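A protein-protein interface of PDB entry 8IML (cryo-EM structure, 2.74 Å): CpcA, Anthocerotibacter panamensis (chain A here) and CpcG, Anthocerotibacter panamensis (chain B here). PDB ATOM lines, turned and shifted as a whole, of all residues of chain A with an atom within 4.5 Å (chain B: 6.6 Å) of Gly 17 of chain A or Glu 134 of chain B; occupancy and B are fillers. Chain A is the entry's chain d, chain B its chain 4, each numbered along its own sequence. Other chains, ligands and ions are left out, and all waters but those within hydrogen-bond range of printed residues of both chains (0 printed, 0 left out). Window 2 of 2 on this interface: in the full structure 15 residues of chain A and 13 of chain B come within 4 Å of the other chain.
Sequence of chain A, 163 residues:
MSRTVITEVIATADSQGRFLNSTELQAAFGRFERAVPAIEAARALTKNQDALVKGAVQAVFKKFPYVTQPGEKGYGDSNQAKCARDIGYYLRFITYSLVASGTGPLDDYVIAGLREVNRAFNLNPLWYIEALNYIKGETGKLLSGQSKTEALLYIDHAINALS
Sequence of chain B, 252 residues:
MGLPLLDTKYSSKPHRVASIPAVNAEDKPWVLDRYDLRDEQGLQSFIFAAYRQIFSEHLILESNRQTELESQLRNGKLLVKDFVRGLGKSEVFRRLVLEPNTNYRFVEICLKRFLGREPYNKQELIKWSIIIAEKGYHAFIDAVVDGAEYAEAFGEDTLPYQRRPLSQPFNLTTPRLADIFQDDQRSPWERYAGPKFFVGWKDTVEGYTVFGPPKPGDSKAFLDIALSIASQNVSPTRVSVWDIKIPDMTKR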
ATOM      1  N   ALA A  13     -16.969  -0.511  -1.926  1.00  0.00           N
ATOM      2  CA  ALA A  13     -15.766  -1.089  -2.512  1.00  0.00           C
ATOM      3  C   ALA A  13     -14.904  -0.024  -3.171  1.00  0.00           C
ATOM      4  O   ALA A  13     -13.674  -0.046  -3.055  1.00  0.00           O
ATOM      5  CB  ALA A  13     -16.145  -2.167  -3.520  1.00  0.00           C
ATOM      6  N   ASP A  14     -15.532   0.923  -3.862  1.00  0.00           N
ATOM      7  CA  ASP A  14     -14.810   1.915  -4.645  1.00  0.00           C
ATOM      8  C   ASP A  14     -14.211   3.002  -3.775  1.00  0.00           C
ATOM      9  O   ASP A  14     -13.291   3.703  -4.206  1.00  0.00           O
ATOM     10  CB  ASP A  14     -15.753   2.524  -5.675  1.00  0.00           C
ATOM     11  CG  ASP A  14     -15.028   3.230  -6.780  1.00  0.00           C
ATOM     12  OD1 ASP A  14     -13.789   3.109  -6.853  1.00  0.00           O
ATOM     13  OD2 ASP A  14     -15.698   3.910  -7.581  1.00  0.00           O
ATOM     14  N   SER A  15     -14.718   3.161  -2.558  1.00  0.00           N
ATOM     15  CA  SER A  15     -14.187   4.173  -1.659  1.00  0.00           C
ATOM     16  C   SER A  15     -12.962   3.673  -0.918  1.00  0.00           C
ATOM     17  O   SER A  15     -12.119   4.474  -0.507  1.00  0.00           O
ATOM     18  CB  SER A  15     -15.267   4.599  -0.678  1.00  0.00           C
ATOM     19  OG  SER A  15     -16.382   5.122  -1.366  1.00  0.00           O
ATOM     20  N   GLN A  16     -12.860   2.370  -0.708  1.00  0.00           N
ATOM     21  CA  GLN A  16     -11.642   1.764  -0.201  1.00  0.00           C
ATOM     22  C   GLN A  16     -10.750   1.255  -1.318  1.00  0.00           C
ATOM     23  O   GLN A  16      -9.662   0.748  -1.041  1.00  0.00           O
ATOM     24  CB  GLN A  16     -11.975   0.618   0.752  1.00  0.00           C
ATOM     25  CG  GLN A  16     -12.231   1.057   2.173  1.00  0.00           C
ATOM     26  CD  GLN A  16     -13.700   1.235   2.455  1.00  0.00           C
ATOM     27  OE1 GLN A  16     -14.522   0.421   2.043  1.00  0.00           O
ATOM     28  NE2 GLN A  16     -14.043   2.303   3.159  1.00  0.00           N
ATOM     29  N   GLY A  17     -11.185   1.384  -2.565  1.00  0.00           N
ATOM     30  CA  GLY A  17     -10.392   0.973  -3.700  1.00  0.00           C
ATOM     31  C   GLY A  17     -10.066  -0.499  -3.689  1.00  0.00           C
ATOM     32  O   GLY A  17      -8.910  -0.880  -3.887  1.00  0.00           O
ATOM     33  N   ARG A  18     -11.067  -1.339  -3.454  1.00  0.00           N
ATOM     34  CA  ARG A  18     -10.862  -2.773  -3.393  1.00  0.00           C
ATOM     35  C   ARG A  18     -11.897  -3.490  -4.241  1.00  0.00           C
ATOM     36  O   ARG A  18     -12.903  -2.917  -4.656  1.00  0.00           O
ATOM     37  CB  ARG A  18     -10.932  -3.288  -1.959  1.00  0.00           C
ATOM     38  CG  ARG A  18     -12.294  -3.201  -1.353  1.00  0.00           C
ATOM     39  CD  ARG A  18     -12.225  -3.327   0.149  1.00  0.00           C
ATOM     40  NE  ARG A  18     -13.439  -2.845   0.799  1.00  0.00           N
ATOM     41  CZ  ARG A  18     -14.626  -3.433   0.709  1.00  0.00           C
ATOM     42  NH1 ARG A  18     -14.778  -4.542   0.003  1.00  0.00           N
ATOM     43  NH2 ARG A  18     -15.666  -2.910   1.340  1.00  0.00           N
ATOM     44  N   MET B   1      -0.309   2.181   0.859  1.00  0.00           N
ATOM     45  CA  MET B   1       0.220   3.140  -0.103  1.00  0.00           C
ATOM     46  C   MET B   1       0.633   2.453  -1.399  1.00  0.00           C
ATOM     47  O   MET B   1      -0.198   1.873  -2.097  1.00  0.00           O
ATOM     48  CB  MET B   1       1.405   3.895   0.495  1.00  0.00           C
ATOM     49  CG  MET B   1       1.030   4.781   1.665  1.00  0.00           C
ATOM     50  SD  MET B   1      -0.154   6.051   1.191  1.00  0.00           S
ATOM     51  CE  MET B   1       0.868   7.084   0.146  1.00  0.00           C
ATOM     52  N   GLY B   2       1.913   2.513  -1.711  1.00  0.00           N
ATOM     53  CA  GLY B   2       2.425   1.897  -2.914  1.00  0.00           C
ATOM     54  C   GLY B   2       3.500   2.772  -3.545  1.00  0.00           C
ATOM     55  O   GLY B   2       4.463   3.162  -2.881  1.00  0.00           O
ATOM     56  N   LEU B   3       3.315   3.065  -4.829  1.00  0.00           N
ATOM     57  CA  LEU B   3       4.308   3.804  -5.585  1.00  0.00           C
ATOM     58  C   LEU B   3       4.353   5.261  -5.145  1.00  0.00           C
ATOM     59  O   LEU B   3       3.398   5.777  -4.561  1.00  0.00           O
ATOM     60  CB  LEU B   3       4.003   3.739  -7.077  1.00  0.00           C
ATOM     61  CG  LEU B   3       4.290   2.452  -7.834  1.00  0.00           C
ATOM     62  CD1 LEU B   3       3.642   2.504  -9.185  1.00  0.00           C
ATOM     63  CD2 LEU B   3       5.767   2.288  -7.975  1.00  0.00           C
ATOM     64  N   SER B 129      -5.115  12.227  -9.031  1.00  0.00           N
ATOM     65  CA  SER B 129      -6.217  11.327  -9.332  1.00  0.00           C
ATOM     66  C   SER B 129      -5.851   9.866  -9.149  1.00  0.00           C
ATOM     67  O   SER B 129      -6.745   9.030  -9.006  1.00  0.00           O
ATOM     68  CB  SER B 129      -6.689  11.547 -10.758  1.00  0.00           C
ATOM     69  OG  SER B 129      -5.857  10.854 -11.661  1.00  0.00           O
ATOM     70  N   ILE B 130      -4.563   9.534  -9.156  1.00  0.00           N
ATOM     71  CA  ILE B 130      -4.185   8.138  -8.990  1.00  0.00           C
ATOM     72  C   ILE B 130      -4.475   7.662  -7.577  1.00  0.00           C
ATOM     73  O   ILE B 130      -4.815   6.492  -7.373  1.00  0.00           O
ATOM     74  CB  ILE B 130      -2.714   7.919  -9.373  1.00  0.00           C
ATOM     75  CG1 ILE B 130      -2.460   6.433  -9.580  1.00  0.00           C
ATOM     76  CG2 ILE B 130      -1.789   8.472  -8.315  1.00  0.00           C
ATOM     77  CD1 ILE B 130      -3.466   5.778 -10.477  1.00  0.00           C
ATOM     78  N   ILE B 131      -4.366   8.542  -6.581  1.00  0.00           N
ATOM     79  CA  ILE B 131      -4.707   8.134  -5.225  1.00  0.00           C
ATOM     80  C   ILE B 131      -6.158   7.699  -5.163  1.00  0.00           C
ATOM     81  O   ILE B 131      -6.477   6.649  -4.605  1.00  0.00           O
ATOM     82  CB  ILE B 131      -4.415   9.259  -4.222  1.00  0.00           C
ATOM     83  CG1 ILE B 131      -2.978   9.722  -4.352  1.00  0.00           C
ATOM     84  CG2 ILE B 131      -4.645   8.773  -2.821  1.00  0.00           C
ATOM     85  CD1 ILE B 131      -2.609  10.742  -3.347  1.00  0.00           C
ATOM     86  N   ILE B 132      -7.056   8.481  -5.756  1.00  0.00           N
ATOM     87  CA  ILE B 132      -8.441   8.046  -5.859  1.00  0.00           C
ATOM     88  C   ILE B 132      -8.516   6.722  -6.593  1.00  0.00           C
ATOM     89  O   ILE B 132      -8.920   5.708  -6.019  1.00  0.00           O
ATOM     90  CB  ILE B 132      -9.290   9.117  -6.561  1.00  0.00           C
ATOM     91  CG1 ILE B 132      -8.957  10.498  -6.030  1.00  0.00           C
ATOM     92  CG2 ILE B 132     -10.758   8.839  -6.371  1.00  0.00           C
ATOM     93  CD1 ILE B 132      -9.393  11.561  -6.948  1.00  0.00           C
ATOM     94  N   ALA B 133      -8.017   6.692  -7.828  1.00  0.00           N
ATOM     95  CA  ALA B 133      -8.210   5.550  -8.711  1.00  0.00           C
ATOM     96  C   ALA B 133      -7.734   4.251  -8.083  1.00  0.00           C
ATOM     97  O   ALA B 133      -8.275   3.183  -8.377  1.00  0.00           O
ATOM     98  CB  ALA B 133      -7.476   5.796 -10.020  1.00  0.00           C
ATOM     99  N   GLU B 134      -6.731   4.318  -7.216  1.00  0.00           N
ATOM    100  CA  GLU B 134      -6.089   3.117  -6.712  1.00  0.00           C
ATOM    101  C   GLU B 134      -6.380   2.817  -5.254  1.00  0.00           C
ATOM    102  O   GLU B 134      -6.281   1.660  -4.852  1.00  0.00           O
ATOM    103  CB  GLU B 134      -4.575   3.226  -6.904  1.00  0.00           C
ATOM    104  CG  GLU B 134      -3.804   1.970  -6.585  1.00  0.00           C
ATOM    105  CD  GLU B 134      -2.376   2.259  -6.191  1.00  0.00           C
ATOM    106  OE1 GLU B 134      -1.583   1.301  -6.092  1.00  0.00           O
ATOM    107  OE2 GLU B 134      -2.044   3.444  -5.985  1.00  0.00           O
ATOM    108  N   LYS B 135      -6.750   3.812  -4.445  1.00  0.00           N
ATOM    109  CA  LYS B 135      -6.913   3.607  -3.016  1.00  0.00           C
ATOM    110  C   LYS B 135      -8.194   4.215  -2.466  1.00  0.00           C
ATOM    111  O   LYS B 135      -8.373   4.225  -1.247  1.00  0.00           O
ATOM    112  CB  LYS B 135      -5.732   4.196  -2.245  1.00  0.00           C
ATOM    113  CG  LYS B 135      -4.369   3.813  -2.752  1.00  0.00           C
ATOM    114  CD  LYS B 135      -3.299   4.581  -2.008  1.00  0.00           C
ATOM    115  CE  LYS B 135      -1.978   4.540  -2.751  1.00  0.00           C
ATOM    116  NZ  LYS B 135      -0.963   5.425  -2.120  1.00  0.00           N
ATOM    117  N   GLY B 136      -9.081   4.729  -3.304  1.00  0.00           N
ATOM    118  CA  GLY B 136     -10.289   5.342  -2.808  1.00  0.00           C
ATOM    119  C   GLY B 136     -10.139   6.826  -2.523  1.00  0.00           C
ATOM    120  O   GLY B 136      -9.073   7.336  -2.160  1.00  0.00           O
ATOM    121  N   TYR B 137     -11.252   7.532  -2.663  1.00  0.00           N
ATOM    122  CA  TYR B 137     -11.221   8.946  -2.352  1.00  0.00           C
ATOM    123  C   TYR B 137     -11.064   9.188  -0.861  1.00  0.00           C
ATOM    124  O   TYR B 137     -10.676  10.286  -0.470  1.00  0.00           O
ATOM    125  CB  TYR B 137     -12.470   9.643  -2.892  1.00  0.00           C
ATOM    126  CG  TYR B 137     -13.650   9.673  -1.960  1.00  0.00           C
ATOM    127  CD1 TYR B 137     -14.407   8.546  -1.737  1.00  0.00           C
ATOM    128  CD2 TYR B 137     -14.023  10.846  -1.331  1.00  0.00           C
ATOM    129  CE1 TYR B 137     -15.484   8.578  -0.897  1.00  0.00           C
ATOM    130  CE2 TYR B 137     -15.102  10.886  -0.490  1.00  0.00           C
ATOM    131  CZ  TYR B 137     -15.828   9.750  -0.277  1.00  0.00           C
ATOM    132  OH  TYR B 137     -16.911   9.783   0.566  1.00  0.00           O
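Among the printed residues, pairs that only touch across the chains: Asp 14 of chain A with Gly 136 of chain B, Ser 15 of chain A with Lys 135 of chain B, Ser 15 of chain A with Gly 136 of chain B, Ser 15 of chain A with Tyr 137 of chain B, Gln 16 of chain A with Lys 135 of chain B, Gly 17 of chain A with Glu 134 of chain B and Gly 17 of chain A with Gly 136 of chain B.
Printed residues of chain B that touch a printed residue of chain A: Glu 134, Lys 135, Gly 136 and Tyr 137. Hydrophobic or aromatic side chains of chain B that line the printed part of chain A: Tyr 137. Printed residues of chain A that touch a printed residue of chain B: Asp 14, Ser 15, Gln 16 and Gly 17.
O of Ile 131 of chain B lies within hydrogen-bond range of N of Gly 136 of chain B, at 3.5 Å. The side-chain sulfur of Met 1 of chain B sits close to the side-chain amino group of Lys 135 of chain B (3.5 Å).
Of chain A, only Gly 17 comes within 4 Å of Glu 134 of chain B. Of the printed residues of chain A, Tyr 137 of chain B touches Ser 15 (3.6 Å). Of the printed residues of chain A, Lys 135 of chain B touches Ser 15 (3.8 Å) and Gln 16 (3.7 Å). Ala 133 of chain B touches none of the printed residues of chain A. Arg 18 of chain A touches none of the printed residues of chain B. The nearest printed residue of chain A that does not touch Glu 134 of chain B is Gln 16 of chain A (5.2 Å). The nearest printed residue of chain A that does not touch Lys 135 of chain B is Gly 17 of chain A (4.1 Å).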
